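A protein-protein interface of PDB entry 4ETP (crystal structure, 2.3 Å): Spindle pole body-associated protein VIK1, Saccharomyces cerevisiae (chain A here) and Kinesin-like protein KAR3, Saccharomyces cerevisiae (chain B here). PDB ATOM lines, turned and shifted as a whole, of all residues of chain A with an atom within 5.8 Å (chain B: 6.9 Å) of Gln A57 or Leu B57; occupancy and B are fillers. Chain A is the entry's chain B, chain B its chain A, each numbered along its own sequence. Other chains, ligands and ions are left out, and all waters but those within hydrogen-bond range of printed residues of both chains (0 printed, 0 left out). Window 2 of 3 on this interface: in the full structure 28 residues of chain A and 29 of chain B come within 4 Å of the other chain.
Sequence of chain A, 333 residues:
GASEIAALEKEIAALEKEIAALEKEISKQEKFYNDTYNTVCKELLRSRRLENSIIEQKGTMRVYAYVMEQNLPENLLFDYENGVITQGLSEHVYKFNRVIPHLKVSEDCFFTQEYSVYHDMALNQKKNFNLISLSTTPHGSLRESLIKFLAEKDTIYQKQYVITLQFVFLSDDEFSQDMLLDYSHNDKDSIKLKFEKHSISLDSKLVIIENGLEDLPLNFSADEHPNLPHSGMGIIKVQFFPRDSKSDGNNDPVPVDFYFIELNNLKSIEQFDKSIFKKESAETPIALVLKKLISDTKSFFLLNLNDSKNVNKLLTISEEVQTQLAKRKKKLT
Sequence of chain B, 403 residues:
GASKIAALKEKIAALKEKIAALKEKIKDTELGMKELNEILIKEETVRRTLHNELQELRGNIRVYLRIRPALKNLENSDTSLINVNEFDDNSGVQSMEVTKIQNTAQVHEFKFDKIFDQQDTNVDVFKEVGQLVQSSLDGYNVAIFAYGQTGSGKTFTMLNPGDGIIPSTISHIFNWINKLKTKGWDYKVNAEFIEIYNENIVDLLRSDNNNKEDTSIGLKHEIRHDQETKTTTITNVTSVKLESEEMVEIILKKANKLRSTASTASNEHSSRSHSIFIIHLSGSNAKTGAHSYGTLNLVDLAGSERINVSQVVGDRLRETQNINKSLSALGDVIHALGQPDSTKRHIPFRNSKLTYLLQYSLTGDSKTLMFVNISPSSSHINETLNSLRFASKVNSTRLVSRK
The guanidinium group (NE) of Arg B62 lies within hydrogen-bond range of the backbone carbonyl oxygen (O) of Arg B58 (3.5 Å).
Of the printed residues of chain B, Ser A53 touches Leu B54 (3.8 Å).
Printed residues of chain B within 4 Å of Ile A54: Leu B50 (3.5 Å), Glu B53 (3.6 Å), Leu B54 (3.97 Å) and Leu B57 (3.8 Å).
Gln A57 touches just these residues of chain B: Leu B54, Leu B57 and Arg B58.
Asn B90 touches none of the printed residues of chain A.
The nearest residue of chain B that does not touch Gln A57 is Gly B92 (6.4 Å).
The nearest printed residue of chain B that does not touch Ser A53 is Arg B58 (4.02 Å).
Among the printed residues, pairs that only touch across the chains: Ser A53 with Leu B54 (3.8 Å), Ile A54 with Leu B50 (3.5 Å), Ile A54 with Glu B53 (3.6 Å), Ile A54 with Leu B54 (3.97 Å), Ile A54 with Leu B57 (3.8 Å), Gln A57 with Leu B54 (3.9 Å), Gln A57 with Arg B58 (3.6 Å) and Lys A58 with Leu B57 (3.9 Å).
The side-chain carboxylate (OE2) of Glu B53 is in salt-bridge range of the side-chain amino group (NZ) of Lys A58 (3.2 Å).
O of Leu B57 is in hydrogen-bond range of NE2 of Gln A57 (3.5 Å).
Hydrophobic or aromatic side chains of chain A within 4 Å of the printed part of chain B: Ile A54.
Printed residues of chain B that touch a printed residue of chain A: Leu B50, Glu B53, Leu B54, Leu B57 and Arg B58.
Hydrophobic or aromatic side chains of chain B within 4 Å of the printed part of chain A: Leu B50, Leu B54 and Leu B57.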
ATOM      1  N   ASN A  52      16.584 -24.627  -1.186  1.00  0.00           N
ATOM      2  CA  ASN A  52      15.351 -24.132  -0.576  1.00  0.00           C
ATOM      3  C   ASN A  52      15.148 -22.635  -0.785  1.00  0.00           C
ATOM      4  O   ASN A  52      14.033 -22.190  -1.061  1.00  0.00           O
ATOM      5  CB  ASN A  52      15.300 -24.452   0.915  1.00  0.00           C
ATOM      6  CG  ASN A  52      13.918 -24.240   1.501  1.00  0.00           C
ATOM      7  OD1 ASN A  52      12.971 -24.936   1.137  1.00  0.00           O
ATOM      8  ND2 ASN A  52      13.793 -23.270   2.401  1.00  0.00           N
ATOM      9  N   SER A  53      16.231 -21.871  -0.655  1.00  0.00           N
ATOM     10  CA  SER A  53      16.205 -20.433  -0.903  1.00  0.00           C
ATOM     11  C   SER A  53      15.879 -20.115  -2.358  1.00  0.00           C
ATOM     12  O   SER A  53      15.241 -19.104  -2.646  1.00  0.00           O
ATOM     13  CB  SER A  53      17.539 -19.794  -0.518  1.00  0.00           C
ATOM     14  OG  SER A  53      17.674 -19.724   0.886  1.00  0.00           O
ATOM     15  N   ILE A  54      16.322 -20.983  -3.267  1.00  0.00           N
ATOM     16  CA  ILE A  54      16.027 -20.832  -4.693  1.00  0.00           C
ATOM     17  C   ILE A  54      14.543 -21.098  -4.963  1.00  0.00           C
ATOM     18  O   ILE A  54      13.901 -20.346  -5.696  1.00  0.00           O
ATOM     19  CB  ILE A  54      16.959 -21.710  -5.567  1.00  0.00           C
ATOM     20  CG1 ILE A  54      18.381 -21.137  -5.553  1.00  0.00           C
ATOM     21  CG2 ILE A  54      16.464 -21.791  -7.004  1.00  0.00           C
ATOM     22  CD1 ILE A  54      19.458 -22.125  -5.954  1.00  0.00           C
ATOM     23  N   ILE A  55      13.999 -22.145  -4.345  1.00  0.00           N
ATOM     24  CA  ILE A  55      12.573 -22.471  -4.469  1.00  0.00           C
ATOM     25  C   ILE A  55      11.687 -21.321  -3.972  1.00  0.00           C
ATOM     26  O   ILE A  55      10.680 -20.993  -4.600  1.00  0.00           O
ATOM     27  CB  ILE A  55      12.217 -23.797  -3.749  1.00  0.00           C
ATOM     28  CG1 ILE A  55      12.866 -24.981  -4.473  1.00  0.00           C
ATOM     29  CG2 ILE A  55      10.705 -23.994  -3.683  1.00  0.00           C
ATOM     30  CD1 ILE A  55      12.993 -26.234  -3.633  1.00  0.00           C
ATOM     31  N   GLU A  56      12.078 -20.709  -2.854  1.00  0.00           N
ATOM     32  CA  GLU A  56      11.363 -19.560  -2.292  1.00  0.00           C
ATOM     33  C   GLU A  56      11.365 -18.351  -3.225  1.00  0.00           C
ATOM     34  O   GLU A  56      10.343 -17.683  -3.379  1.00  0.00           O
ATOM     35  CB  GLU A  56      11.952 -19.165  -0.936  1.00  0.00           C
ATOM     36  CG  GLU A  56      11.609 -20.124   0.189  1.00  0.00           C
ATOM     37  CD  GLU A  56      10.125 -20.147   0.502  1.00  0.00           C
ATOM     38  OE1 GLU A  56       9.594 -19.109   0.954  1.00  0.00           O
ATOM     39  OE2 GLU A  56       9.494 -21.207   0.301  1.00  0.00           O
ATOM     40  N   GLN A  57      12.516 -18.078  -3.836  1.00  0.00           N
ATOM     41  CA  GLN A  57      12.659 -16.963  -4.771  1.00  0.00           C
ATOM     42  C   GLN A  57      11.787 -17.146  -6.007  1.00  0.00           C
ATOM     43  O   GLN A  57      11.079 -16.227  -6.415  1.00  0.00           O
ATOM     44  CB  GLN A  57      14.124 -16.784  -5.184  1.00  0.00           C
ATOM     45  CG  GLN A  57      14.999 -16.090  -4.148  1.00  0.00           C
ATOM     46  CD  GLN A  57      14.779 -14.587  -4.081  1.00  0.00           C
ATOM     47  OE1 GLN A  57      15.045 -13.958  -3.057  1.00  0.00           O
ATOM     48  NE2 GLN A  57      14.296 -14.004  -5.172  1.00  0.00           N
ATOM     49  N   LYS A  58      11.838 -18.340  -6.590  1.00  0.00           N
ATOM     50  CA  LYS A  58      11.080 -18.642  -7.802  1.00  0.00           C
ATOM     51  C   LYS A  58       9.592 -18.836  -7.521  1.00  0.00           C
ATOM     52  O   LYS A  58       8.761 -18.672  -8.416  1.00  0.00           O
ATOM     53  CB  LYS A  58      11.664 -19.867  -8.516  1.00  0.00           C
ATOM     54  CG  LYS A  58      13.063 -19.640  -9.074  1.00  0.00           C
ATOM     55  CD  LYS A  58      13.438 -20.639 -10.159  1.00  0.00           C
ATOM     56  CE  LYS A  58      13.887 -21.972  -9.583  1.00  0.00           C
ATOM     57  NZ  LYS A  58      14.802 -22.690 -10.514  1.00  0.00           N
ATOM     58  N   GLY A  59       9.265 -19.183  -6.279  1.00  0.00           N
ATOM     59  CA  GLY A  59       7.877 -19.377  -5.852  1.00  0.00           C
ATOM     60  C   GLY A  59       7.215 -20.618  -6.424  1.00  0.00           C
ATOM     61  O   GLY A  59       5.989 -20.724  -6.428  1.00  0.00           O
ATOM     62  N   LEU B  50      24.807 -23.401  -7.506  1.00  0.00           N
ATOM     63  CA  LEU B  50      23.587 -23.049  -6.777  1.00  0.00           C
ATOM     64  C   LEU B  50      23.652 -21.636  -6.199  1.00  0.00           C
ATOM     65  O   LEU B  50      22.679 -20.880  -6.286  1.00  0.00           O
ATOM     66  CB  LEU B  50      23.288 -24.069  -5.674  1.00  0.00           C
ATOM     67  CG  LEU B  50      22.839 -25.474  -6.108  1.00  0.00           C
ATOM     68  CD1 LEU B  50      22.833 -26.419  -4.917  1.00  0.00           C
ATOM     69  CD2 LEU B  50      21.470 -25.449  -6.775  1.00  0.00           C
ATOM     70  N   ASN B  52      25.394 -19.060  -7.272  1.00  0.00           N
ATOM     71  CA  ASN B  52      25.255 -18.059  -8.329  1.00  0.00           C
ATOM     72  C   ASN B  52      23.825 -17.898  -8.818  1.00  0.00           C
ATOM     73  O   ASN B  52      23.382 -16.776  -9.081  1.00  0.00           O
ATOM     74  CB  ASN B  52      26.184 -18.320  -9.517  1.00  0.00           C
ATOM     75  CG  ASN B  52      26.235 -17.137 -10.472  1.00  0.00           C
ATOM     76  OD1 ASN B  52      26.716 -16.058 -10.118  1.00  0.00           O
ATOM     77  ND2 ASN B  52      25.725 -17.328 -11.681  1.00  0.00           N
ATOM     78  N   GLU B  53      23.104 -19.013  -8.925  1.00  0.00           N
ATOM     79  CA  GLU B  53      21.690 -18.974  -9.289  1.00  0.00           C
ATOM     80  C   GLU B  53      20.895 -18.126  -8.299  1.00  0.00           C
ATOM     81  O   GLU B  53      20.068 -17.310  -8.710  1.00  0.00           O
ATOM     82  CB  GLU B  53      21.093 -20.385  -9.401  1.00  0.00           C
ATOM     83  CG  GLU B  53      19.646 -20.388  -9.886  1.00  0.00           C
ATOM     84  CD  GLU B  53      19.026 -21.772 -10.009  1.00  0.00           C
ATOM     85  OE1 GLU B  53      19.624 -22.765  -9.541  1.00  0.00           O
ATOM     86  OE2 GLU B  53      17.919 -21.863 -10.583  1.00  0.00           O
ATOM     87  N   LEU B  54      21.165 -18.308  -7.005  1.00  0.00           N
ATOM     88  CA  LEU B  54      20.500 -17.533  -5.957  1.00  0.00           C
ATOM     89  C   LEU B  54      20.830 -16.048  -6.088  1.00  0.00           C
ATOM     90  O   LEU B  54      19.954 -15.196  -5.926  1.00  0.00           O
ATOM     91  CB  LEU B  54      20.921 -18.019  -4.565  1.00  0.00           C
ATOM     92  CG  LEU B  54      19.884 -18.129  -3.435  1.00  0.00           C
ATOM     93  CD1 LEU B  54      20.571 -18.037  -2.075  1.00  0.00           C
ATOM     94  CD2 LEU B  54      18.739 -17.128  -3.521  1.00  0.00           C
ATOM     95  N   GLN B  55      22.101 -15.752  -6.365  1.00  0.00           N
ATOM     96  CA  GLN B  55      22.567 -14.379  -6.544  1.00  0.00           C
ATOM     97  C   GLN B  55      21.891 -13.695  -7.728  1.00  0.00           C
ATOM     98  O   GLN B  55      21.555 -12.511  -7.654  1.00  0.00           O
ATOM     99  CB  GLN B  55      24.098 -14.322  -6.683  1.00  0.00           C
ATOM    100  CG  GLN B  55      24.850 -14.774  -5.436  1.00  0.00           C
ATOM    101  CD  GLN B  55      24.288 -14.160  -4.164  1.00  0.00           C
ATOM    102  OE1 GLN B  55      24.283 -12.940  -3.998  1.00  0.00           O
ATOM    103  NE2 GLN B  55      23.800 -15.007  -3.262  1.00  0.00           N
ATOM    104  N   GLU B  56      21.692 -14.440  -8.811  1.00  0.00           N
ATOM    105  CA  GLU B  56      20.976 -13.919  -9.977  1.00  0.00           C
ATOM    106  C   GLU B  56      19.535 -13.573  -9.613  1.00  0.00           C
ATOM    107  O   GLU B  56      19.067 -12.469  -9.894  1.00  0.00           O
ATOM    108  CB  GLU B  56      21.007 -14.921 -11.131  1.00  0.00           C
ATOM    109  CG  GLU B  56      22.366 -15.052 -11.798  1.00  0.00           C
ATOM    110  CD  GLU B  56      22.403 -16.144 -12.854  1.00  0.00           C
ATOM    111  OE1 GLU B  56      21.727 -17.184 -12.682  1.00  0.00           O
ATOM    112  OE2 GLU B  56      23.125 -15.965 -13.855  1.00  0.00           O
ATOM    113  N   LEU B  57      18.853 -14.512  -8.959  1.00  0.00           N
ATOM    114  CA  LEU B  57      17.461 -14.338  -8.540  1.00  0.00           C
ATOM    115  C   LEU B  57      17.264 -13.169  -7.575  1.00  0.00           C
ATOM    116  O   LEU B  57      16.233 -12.495  -7.614  1.00  0.00           O
ATOM    117  CB  LEU B  57      16.921 -15.632  -7.926  1.00  0.00           C
ATOM    118  CG  LEU B  57      16.734 -16.811  -8.889  1.00  0.00           C
ATOM    119  CD1 LEU B  57      16.666 -18.121  -8.121  1.00  0.00           C
ATOM    120  CD2 LEU B  57      15.496 -16.636  -9.766  1.00  0.00           C
ATOM    121  N   ARG B  58      18.255 -12.934  -6.719  1.00  0.00           N
ATOM    122  CA  ARG B  58      18.230 -11.804  -5.792  1.00  0.00           C
ATOM    123  C   ARG B  58      18.682 -10.502  -6.463  1.00  0.00           C
ATOM    124  O   ARG B  58      18.549  -9.421  -5.888  1.00  0.00           O
ATOM    125  CB  ARG B  58      19.081 -12.104  -4.554  1.00  0.00           C
ATOM    126  CG  ARG B  58      18.468 -13.165  -3.650  1.00  0.00           C
ATOM    127  CD  ARG B  58      19.342 -13.470  -2.446  1.00  0.00           C
ATOM    128  NE  ARG B  58      18.661 -14.387  -1.543  1.00  0.00           N
ATOM    129  CZ  ARG B  58      19.237 -15.034  -0.534  1.00  0.00           C
ATOM    130  NH1 ARG B  58      20.529 -14.879  -0.281  1.00  0.00           N
ATOM    131  NH2 ARG B  58      18.512 -15.847   0.220  1.00  0.00           N
ATOM    132  N   GLY B  59      19.210 -10.616  -7.677  1.00  0.00           N
ATOM    133  CA  GLY B  59      19.606  -9.453  -8.463  1.00  0.00           C
ATOM    134  C   GLY B  59      21.107  -9.239  -8.513  1.00  0.00           C
ATOM    135  O   GLY B  59      21.772  -9.205  -7.473  1.00  0.00           O
ATOM    136  N   ASN B  60      21.636  -9.098  -9.729  1.00  0.00           N
ATOM    137  CA  ASN B  60      23.044  -8.771  -9.974  1.00  0.00           C
ATOM    138  C   ASN B  60      23.377  -7.330  -9.581  1.00  0.00           C
ATOM    139  O   ASN B  60      24.540  -6.964  -9.416  1.00  0.00           O
ATOM    140  CB  ASN B  60      23.395  -9.008 -11.452  1.00  0.00           C
ATOM    141  CG  ASN B  60      22.598  -8.120 -12.407  1.00  0.00           C
ATOM    142  OD1 ASN B  60      21.483  -7.692 -12.103  1.00  0.00           O
ATOM    143  ND2 ASN B  60      23.173  -7.850 -13.575  1.00  0.00           N
ATOM    144  N   ARG B  62      22.082  -4.570  -6.691  1.00  0.00           N
ATOM    145  CA  ARG B  62      21.296  -4.371  -5.472  1.00  0.00           C
ATOM    146  C   ARG B  62      21.591  -3.018  -4.843  1.00  0.00           C
ATOM    147  O   ARG B  62      22.706  -2.507  -4.943  1.00  0.00           O
ATOM    148  CB  ARG B  62      21.585  -5.477  -4.453  1.00  0.00           C
ATOM    149  CG  ARG B  62      21.073  -6.847  -4.851  1.00  0.00           C
ATOM    150  CD  ARG B  62      21.690  -7.939  -3.991  1.00  0.00           C
ATOM    151  NE  ARG B  62      21.841  -9.163  -4.770  1.00  0.00           N
ATOM    152  CZ  ARG B  62      22.506 -10.245  -4.380  1.00  0.00           C
ATOM    153  NH1 ARG B  62      23.096 -10.292  -3.192  1.00  0.00           N
ATOM    154  NH2 ARG B  62      22.573 -11.294  -5.188  1.00  0.00           N
ATOM    155  N   ASN B  90       7.181 -10.960   0.393  1.00  0.00           N
ATOM    156  CA  ASN B  90       6.561 -11.350  -0.869  1.00  0.00           C
ATOM    157  C   ASN B  90       7.225 -10.709  -2.090  1.00  0.00           C
ATOM    158  O   ASN B  90       7.566 -11.402  -3.050  1.00  0.00           O
ATOM    159  CB  ASN B  90       5.058 -11.039  -0.845  1.00  0.00           C
ATOM    160  CG  ASN B  90       4.291 -11.743  -1.952  1.00  0.00           C
ATOM    161  OD1 ASN B  90       4.555 -12.904  -2.272  1.00  0.00           O
ATOM    162  ND2 ASN B  90       3.323 -11.043  -2.533  1.00  0.00           N
ATOM    163  N   GLY B  92      10.088  -8.817  -1.997  1.00  0.00           N
ATOM    164  CA  GLY B  92      11.539  -8.712  -1.814  1.00  0.00           C
ATOM    165  C   GLY B  92      12.052  -7.284  -1.707  1.00  0.00           C
ATOM    166  O   GLY B  92      13.258  -7.044  -1.769  1.00  0.00           O
